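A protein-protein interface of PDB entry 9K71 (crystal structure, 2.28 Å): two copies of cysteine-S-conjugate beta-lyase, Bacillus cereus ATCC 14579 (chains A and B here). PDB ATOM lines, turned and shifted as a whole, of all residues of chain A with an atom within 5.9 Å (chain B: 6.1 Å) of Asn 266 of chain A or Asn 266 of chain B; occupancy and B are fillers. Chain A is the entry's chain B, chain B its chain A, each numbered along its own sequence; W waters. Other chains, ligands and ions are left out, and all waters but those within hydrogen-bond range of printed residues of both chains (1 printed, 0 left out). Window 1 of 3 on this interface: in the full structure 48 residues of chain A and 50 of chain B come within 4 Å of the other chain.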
ATOM      1  N   THR A  58      36.587 -15.920  29.515  1.00  0.00           N
ATOM      2  CA  THR A  58      37.393 -16.030  28.318  1.00  0.00           C
ATOM      3  C   THR A  58      36.938 -15.011  27.296  1.00  0.00           C
ATOM      4  O   THR A  58      35.744 -14.717  27.172  1.00  0.00           O
ATOM      5  CB  THR A  58      37.392 -17.459  27.728  1.00  0.00           C
ATOM      6  OG1 THR A  58      36.155 -17.741  27.061  1.00  0.00           O
ATOM      7  CG2 THR A  58      37.710 -18.503  28.825  1.00  0.00           C
ATOM      8  N   GLY A 236      20.891 -24.304  23.471  1.00  0.00           N
ATOM      9  CA  GLY A 236      21.218 -24.275  24.885  1.00  0.00           C
ATOM     10  C   GLY A 236      22.634 -23.832  25.175  1.00  0.00           C
ATOM     11  O   GLY A 236      23.054 -23.756  26.338  1.00  0.00           O
ATOM     12  N   LEU A 237      23.389 -23.548  24.115  1.00  0.00           N
ATOM     13  CA  LEU A 237      24.694 -22.954  24.292  1.00  0.00           C
ATOM     14  C   LEU A 237      24.625 -21.435  24.220  1.00  0.00           C
ATOM     15  O   LEU A 237      25.564 -20.763  24.669  1.00  0.00           O
ATOM     16  CB  LEU A 237      25.655 -23.521  23.255  1.00  0.00           C
ATOM     17  CG  LEU A 237      25.641 -25.052  23.187  1.00  0.00           C
ATOM     18  CD1 LEU A 237      26.708 -25.553  22.262  1.00  0.00           C
ATOM     19  CD2 LEU A 237      25.848 -25.648  24.562  1.00  0.00           C
ATOM     20  N   GLN A 238      23.525 -20.889  23.693  1.00  0.00           N
ATOM     21  CA  GLN A 238      23.191 -19.472  23.820  1.00  0.00           C
ATOM     22  C   GLN A 238      24.214 -18.598  23.096  1.00  0.00           C
ATOM     23  O   GLN A 238      24.828 -17.689  23.667  1.00  0.00           O
ATOM     24  CB  GLN A 238      23.044 -19.077  25.296  1.00  0.00           C
ATOM     25  CG  GLN A 238      21.736 -19.607  25.905  1.00  0.00           C
ATOM     26  CD  GLN A 238      21.530 -19.251  27.388  1.00  0.00           C
ATOM     27  OE1 GLN A 238      22.473 -18.985  28.139  1.00  0.00           O
ATOM     28  NE2 GLN A 238      20.275 -19.257  27.808  1.00  0.00           N
ATOM     29  N   GLY A 264      29.497 -10.798  27.259  1.00  0.00           N
ATOM     30  CA  GLY A 264      29.852 -11.735  26.216  1.00  0.00           C
ATOM     31  C   GLY A 264      29.487 -13.173  26.526  1.00  0.00           C
ATOM     32  O   GLY A 264      29.167 -13.552  27.653  1.00  0.00           O
ATOM     33  N   LEU A 265      29.622 -13.993  25.487  1.00  0.00           N
ATOM     34  CA  LEU A 265      29.194 -15.382  25.471  1.00  0.00           C
ATOM     35  C   LEU A 265      29.952 -16.257  26.460  1.00  0.00           C
ATOM     36  O   LEU A 265      31.053 -15.926  26.951  1.00  0.00           O
ATOM     37  CB  LEU A 265      29.361 -15.940  24.064  1.00  0.00           C
ATOM     38  CG  LEU A 265      28.571 -15.027  23.118  1.00  0.00           C
ATOM     39  CD1 LEU A 265      28.499 -15.596  21.704  1.00  0.00           C
ATOM     40  CD2 LEU A 265      27.151 -14.766  23.683  1.00  0.00           C
ATOM     41  N   ASN A 266      29.345 -17.411  26.733  1.00  0.00           N
ATOM     42  CA  ASN A 266      30.005 -18.365  27.600  1.00  0.00           C
ATOM     43  C   ASN A 266      31.033 -19.118  26.779  1.00  0.00           C
ATOM     44  O   ASN A 266      31.017 -19.099  25.538  1.00  0.00           O
ATOM     45  CB  ASN A 266      29.002 -19.305  28.340  1.00  0.00           C
ATOM     46  CG  ASN A 266      28.297 -20.348  27.422  1.00  0.00           C
ATOM     47  OD1 ASN A 266      28.788 -21.481  27.227  1.00  0.00           O
ATOM     48  ND2 ASN A 266      27.114 -19.983  26.916  1.00  0.00           N
ATOM     49  N   ILE A 267      31.967 -19.739  27.508  1.00  0.00           N
ATOM     50  CA  ILE A 267      33.135 -20.378  26.906  1.00  0.00           C
ATOM     51  C   ILE A 267      32.724 -21.309  25.767  1.00  0.00           C
ATOM     52  O   ILE A 267      33.376 -21.360  24.717  1.00  0.00           O
ATOM     53  CB  ILE A 267      33.920 -21.129  28.000  1.00  0.00           C
ATOM     54  CG1 ILE A 267      34.642 -20.171  28.924  1.00  0.00           C
ATOM     55  CG2 ILE A 267      34.936 -22.036  27.430  1.00  0.00           C
ATOM     56  CD1 ILE A 267      35.323 -20.906  30.015  1.00  0.00           C
ATOM     57  N   PHE A 268      31.631 -22.046  25.953  1.00  0.00           N
ATOM     58  CA  PHE A 268      31.208 -23.096  25.032  1.00  0.00           C
ATOM     59  C   PHE A 268      30.351 -22.580  23.891  1.00  0.00           C
ATOM     60  O   PHE A 268      30.164 -23.294  22.895  1.00  0.00           O
ATOM     61  CB  PHE A 268      30.453 -24.184  25.798  1.00  0.00           C
ATOM     62  CG  PHE A 268      31.321 -24.971  26.745  1.00  0.00           C
ATOM     63  CD1 PHE A 268      32.289 -25.833  26.259  1.00  0.00           C
ATOM     64  CD2 PHE A 268      31.176 -24.839  28.117  1.00  0.00           C
ATOM     65  CE1 PHE A 268      33.085 -26.564  27.124  1.00  0.00           C
ATOM     66  CE2 PHE A 268      31.959 -25.564  28.980  1.00  0.00           C
ATOM     67  CZ  PHE A 268      32.919 -26.430  28.485  1.00  0.00           C
ATOM     68  N   ALA A 269      29.770 -21.395  24.033  1.00  0.00           N
ATOM     69  CA  ALA A 269      29.191 -20.743  22.868  1.00  0.00           C
ATOM     70  C   ALA A 269      30.286 -20.433  21.846  1.00  0.00           C
ATOM     71  O   ALA A 269      30.146 -20.723  20.648  1.00  0.00           O
ATOM     72  CB  ALA A 269      28.462 -19.471  23.307  1.00  0.00           C
ATOM     73  N   TYR A 270      31.404 -19.883  22.325  1.00  0.00           N
ATOM     74  CA  TYR A 270      32.550 -19.560  21.478  1.00  0.00           C
ATOM     75  C   TYR A 270      33.134 -20.818  20.840  1.00  0.00           C
ATOM     76  O   TYR A 270      33.335 -20.871  19.626  1.00  0.00           O
ATOM     77  CB  TYR A 270      33.616 -18.845  22.318  1.00  0.00           C
ATOM     78  CG  TYR A 270      33.265 -17.433  22.721  1.00  0.00           C
ATOM     79  CD1 TYR A 270      32.528 -16.624  21.875  1.00  0.00           C
ATOM     80  CD2 TYR A 270      33.694 -16.896  23.945  1.00  0.00           C
ATOM     81  CE1 TYR A 270      32.222 -15.306  22.212  1.00  0.00           C
ATOM     82  CE2 TYR A 270      33.378 -15.561  24.310  1.00  0.00           C
ATOM     83  CZ  TYR A 270      32.631 -14.771  23.425  1.00  0.00           C
ATOM     84  OH  TYR A 270      32.262 -13.459  23.737  1.00  0.00           O
ATOM     85  N   THR A 271      33.461 -21.827  21.653  1.00  0.00           N
ATOM     86  CA  THR A 271      33.985 -23.084  21.112  1.00  0.00           C
ATOM     87  C   THR A 271      33.042 -23.698  20.081  1.00  0.00           C
ATOM     88  O   THR A 271      33.465 -24.079  18.982  1.00  0.00           O
ATOM     89  CB  THR A 271      34.216 -24.092  22.241  1.00  0.00           C
ATOM     90  OG1 THR A 271      34.993 -23.491  23.266  1.00  0.00           O
ATOM     91  CG2 THR A 271      34.922 -25.327  21.740  1.00  0.00           C
ATOM     92  N   THR B  58      16.776 -26.119  27.318  1.00  0.00           N
ATOM     93  CA  THR B  58      16.555 -26.955  28.490  1.00  0.00           C
ATOM     94  C   THR B  58      15.963 -26.171  29.659  1.00  0.00           C
ATOM     95  O   THR B  58      16.210 -24.974  29.823  1.00  0.00           O
ATOM     96  CB  THR B  58      17.842 -27.636  28.985  1.00  0.00           C
ATOM     97  OG1 THR B  58      18.590 -26.724  29.804  1.00  0.00           O
ATOM     98  CG2 THR B  58      18.691 -28.134  27.827  1.00  0.00           C
ATOM     99  N   GLY B 236      33.495 -18.378  33.441  1.00  0.00           N
ATOM    100  CA  GLY B 236      33.144 -18.416  32.055  1.00  0.00           C
ATOM    101  C   GLY B 236      31.971 -19.308  31.712  1.00  0.00           C
ATOM    102  O   GLY B 236      31.603 -19.354  30.539  1.00  0.00           O
ATOM    103  N   LEU B 237      31.356 -20.005  32.675  1.00  0.00           N
ATOM    104  CA  LEU B 237      30.143 -20.764  32.362  1.00  0.00           C
ATOM    105  C   LEU B 237      28.852 -20.048  32.719  1.00  0.00           C
ATOM    106  O   LEU B 237      27.791 -20.460  32.244  1.00  0.00           O
ATOM    107  CB  LEU B 237      30.176 -22.131  33.038  1.00  0.00           C
ATOM    108  CG  LEU B 237      31.428 -22.844  32.542  1.00  0.00           C
ATOM    109  CD1 LEU B 237      31.657 -24.159  33.211  1.00  0.00           C
ATOM    110  CD2 LEU B 237      31.312 -23.011  31.030  1.00  0.00           C
ATOM    111  N   GLN B 238      28.923 -19.005  33.542  1.00  0.00           N
ATOM    112  CA  GLN B 238      27.839 -18.056  33.773  1.00  0.00           C
ATOM    113  C   GLN B 238      26.655 -18.660  34.525  1.00  0.00           C
ATOM    114  O   GLN B 238      25.525 -18.696  34.020  1.00  0.00           O
ATOM    115  CB  GLN B 238      27.412 -17.445  32.429  1.00  0.00           C
ATOM    116  CG  GLN B 238      28.582 -16.739  31.736  1.00  0.00           C
ATOM    117  CD  GLN B 238      28.243 -16.079  30.401  1.00  0.00           C
ATOM    118  OE1 GLN B 238      27.283 -16.452  29.717  1.00  0.00           O
ATOM    119  NE2 GLN B 238      29.043 -15.088  30.022  1.00  0.00           N
ATOM    120  N   GLY B 264      16.912 -18.316  30.778  1.00  0.00           N
ATOM    121  CA  GLY B 264      17.598 -19.256  31.637  1.00  0.00           C
ATOM    122  C   GLY B 264      19.010 -19.551  31.171  1.00  0.00           C
ATOM    123  O   GLY B 264      19.425 -19.211  30.063  1.00  0.00           O
ATOM    124  N   LEU B 265      19.760 -20.188  32.062  1.00  0.00           N
ATOM    125  CA  LEU B 265      21.175 -20.443  31.868  1.00  0.00           C
ATOM    126  C   LEU B 265      21.432 -21.390  30.686  1.00  0.00           C
ATOM    127  O   LEU B 265      20.521 -21.987  30.106  1.00  0.00           O
ATOM    128  CB  LEU B 265      21.787 -20.995  33.152  1.00  0.00           C
ATOM    129  CG  LEU B 265      21.412 -20.246  34.448  1.00  0.00           C
ATOM    130  CD1 LEU B 265      22.239 -20.739  35.642  1.00  0.00           C
ATOM    131  CD2 LEU B 265      21.542 -18.755  34.306  1.00  0.00           C
ATOM    132  N   ASN B 266      22.696 -21.458  30.278  1.00  0.00           N
ATOM    133  CA  ASN B 266      23.060 -22.424  29.259  1.00  0.00           C
ATOM    134  C   ASN B 266      23.255 -23.797  29.899  1.00  0.00           C
ATOM    135  O   ASN B 266      23.540 -23.913  31.090  1.00  0.00           O
ATOM    136  CB  ASN B 266      24.315 -21.974  28.501  1.00  0.00           C
ATOM    137  CG  ASN B 266      25.583 -22.205  29.282  1.00  0.00           C
ATOM    138  OD1 ASN B 266      26.028 -23.350  29.459  1.00  0.00           O
ATOM    139  ND2 ASN B 266      26.182 -21.119  29.758  1.00  0.00           N
ATOM    140  N   ILE B 267      23.164 -24.834  29.057  1.00  0.00           N
ATOM    141  CA  ILE B 267      23.113 -26.233  29.500  1.00  0.00           C
ATOM    142  C   ILE B 267      24.249 -26.562  30.459  1.00  0.00           C
ATOM    143  O   ILE B 267      24.078 -27.331  31.416  1.00  0.00           O
ATOM    144  CB  ILE B 267      23.126 -27.168  28.275  1.00  0.00           C
ATOM    145  CG1 ILE B 267      21.884 -26.945  27.439  1.00  0.00           C
ATOM    146  CG2 ILE B 267      23.198 -28.615  28.666  1.00  0.00           C
ATOM    147  CD1 ILE B 267      21.907 -27.750  26.172  1.00  0.00           C
ATOM    148  N   PHE B 268      25.429 -26.010  30.206  1.00  0.00           N
ATOM    149  CA  PHE B 268      26.591 -26.383  30.992  1.00  0.00           C
ATOM    150  C   PHE B 268      26.684 -25.599  32.284  1.00  0.00           C
ATOM    151  O   PHE B 268      27.375 -26.040  33.210  1.00  0.00           O
ATOM    152  CB  PHE B 268      27.850 -26.177  30.157  1.00  0.00           C
ATOM    153  CG  PHE B 268      27.915 -27.085  28.960  1.00  0.00           C
ATOM    154  CD1 PHE B 268      28.151 -28.431  29.120  1.00  0.00           C
ATOM    155  CD2 PHE B 268      27.714 -26.594  27.685  1.00  0.00           C
ATOM    156  CE1 PHE B 268      28.206 -29.270  28.038  1.00  0.00           C
ATOM    157  CE2 PHE B 268      27.767 -27.423  26.608  1.00  0.00           C
ATOM    158  CZ  PHE B 268      28.012 -28.768  26.778  1.00  0.00           C
ATOM    159  N   ALA B 269      26.002 -24.454  32.360  1.00  0.00           N
ATOM    160  CA  ALA B 269      25.861 -23.756  33.628  1.00  0.00           C
ATOM    161  C   ALA B 269      25.064 -24.598  34.618  1.00  0.00           C
ATOM    162  O   ALA B 269      25.429 -24.700  35.796  1.00  0.00           O
ATOM    163  CB  ALA B 269      25.216 -22.388  33.409  1.00  0.00           C
ATOM    164  N   TYR B 270      23.969 -25.210  34.182  1.00  0.00           N
ATOM    165  CA  TYR B 270      23.183 -26.095  35.077  1.00  0.00           C
ATOM    166  C   TYR B 270      23.987 -27.338  35.465  1.00  0.00           C
ATOM    167  O   TYR B 270      24.058 -27.634  36.646  1.00  0.00           O
ATOM    168  CB  TYR B 270      21.846 -26.462  34.448  1.00  0.00           C
ATOM    169  CG  TYR B 270      20.873 -25.327  34.360  1.00  0.00           C
ATOM    170  CD1 TYR B 270      20.497 -24.632  35.493  1.00  0.00           C
ATOM    171  CD2 TYR B 270      20.343 -24.942  33.144  1.00  0.00           C
ATOM    172  CE1 TYR B 270      19.604 -23.583  35.423  1.00  0.00           C
ATOM    173  CE2 TYR B 270      19.451 -23.893  33.059  1.00  0.00           C
ATOM    174  CZ  TYR B 270      19.077 -23.214  34.203  1.00  0.00           C
ATOM    175  OH  TYR B 270      18.207 -22.171  34.139  1.00  0.00           O
ATOM    176  N   THR B 271      24.560 -28.030  34.475  1.00  0.00           N
ATOM    177  CA  THR B 271      25.337 -29.236  34.759  1.00  0.00           C
ATOM    178  C   THR B 271      26.443 -28.952  35.773  1.00  0.00           C
ATOM    179  O   THR B 271      26.587 -29.674  36.769  1.00  0.00           O
ATOM    180  CB  THR B 271      25.921 -29.812  33.463  1.00  0.00           C
ATOM    181  OG1 THR B 271      24.914 -29.865  32.441  1.00  0.00           O
ATOM    182  CG2 THR B 271      26.460 -31.203  33.691  1.00  0.00           C
HETATM  183  O   HOH W   1      23.855 -19.046  31.282  1.00  0.00           O
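Water W1 lies within hydrogen-bond range of N of Asn 266 of chain B (2.9 Å), O of Gln 238 of chain B (3.2 Å) and OE1 of Gln 238 of chain A (3.4 Å).
Of the 12 printed residues of chain B, 8 touch a printed residue of chain A.
Printed residues of chain B that touch a printed residue of chain A: Gly 236, Leu 237, Gln 238, Gly 264, Leu 265, Asn 266, Ile 267 and Phe 268.
Hydrophobic or aromatic side chains of chain A within 4 Å of the printed part of chain B: Leu 237, Ile 267 and Phe 268.
Among the printed residues, 14 pairs touch across the chains.
Among the printed residues, no Asp or Glu carboxylate lies within 4 Å of a Lys or Arg side-chain nitrogen of the other chain.
Gly 236 of chain A touches Ile 267 of chain B, and with the chains exchanged Ile 267 of chain A touches Gly 236 of chain B.
Gln 238 of chain A touches Gly 264 of chain B, and with the chains exchanged Gly 264 of chain A touches Gln 238 of chain B.
Gln 238 of chain A touches Asn 266 of chain B, and with the chains exchanged Asn 266 of chain A touches Gln 238 of chain B.
Asn 266 of chain B touches its own counterpart, Asn 266 of chain A.
Of the 14 pairs that touch across the chains among the printed residues, 14 have their exchanged pair printed and touching as well.
N of Asn 266 of chain B sits at hydrogen-bond distance from OE1 of Gln 238 of chain A.
The backbone carbonyl oxygen (O) of Gly 264 of chain A sits at hydrogen-bond distance from the side-chain amide nitrogen (NE2) of Gln 238 of chain B (2.8 Å).
O of Gly 236 of chain B sits at hydrogen-bond distance from N of Ile 267 of chain A, 3.1 Å away.
O of Gly 264 of chain B sits at hydrogen-bond distance from NE2 of Gln 238 of chain A (2.4 Å).
The backbone carbonyl oxygen (O) of Gly 236 of chain A sits at hydrogen-bond distance from the backbone NH (N) of Ile 267 of chain B.
The side-chain amide nitrogen (ND2) of Asn 266 of chain B sits close to the side-chain amide nitrogen (ND2) of Asn 266 of chain A (3.2 Å).
The backbone carbonyl oxygen of Leu 237 of chain A lies within hydrogen-bond range of the side-chain amide nitrogen of Asn 266 of chain A (2.8 Å).
OD1 of Asn 266 of chain A lies close to N of Phe 268 of chain A (3.2 Å).
The backbone NH (N) of Ala 269 of chain A sits at hydrogen-bond distance from the side-chain amide oxygen (OD1) of Asn 266 of chain A, at 3.3 Å.
The side-chain hydroxyl of Thr 271 of chain B sits at hydrogen-bond distance from the backbone carbonyl oxygen of Ile 267 of chain B (2.9 Å).
N of Leu 265 of chain B sits at hydrogen-bond distance from OH of Tyr 270 of chain B.
OD1 of Asn 266 of chain B sits at hydrogen-bond distance from N of Ala 269 of chain B (3.1 Å).
Among the printed residues, merely in contact across the chains: Gly 236 of chain A with Asn 266 of chain B, Leu 237 of chain A with Phe 268 of chain B, Gln 238 of chain A with Leu 265 of chain B, Leu 265 of chain A with Gln 238 of chain B, Asn 266 of chain A with Gly 236 of chain B, Asn 266 of chain A with Gln 238 of chain B, Phe 268 of chain A with Leu 237 of chain B and Phe 268 of chain A with Phe 268 of chain B.
Of the printed residues of chain B, Gly 264 of chain A touches Gln 238 (2.8 Å).
Printed residues of chain B within 4 Å of Ile 267 of chain A: Gly 236 (3.1 Å).
Of the printed residues of chain B, Phe 268 of chain A touches Leu 237 and Phe 268.
Of the printed residues of chain A, Ile 267 of chain B touches Gly 236 (2.9 Å).
The nearest residue of chain A that does not touch Asn 266 of chain B is Leu 237 of chain A (4.2 Å).
The nearest printed residue of chain B that does not touch Leu 237 of chain A is Asn 266 of chain B (4.2 Å).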
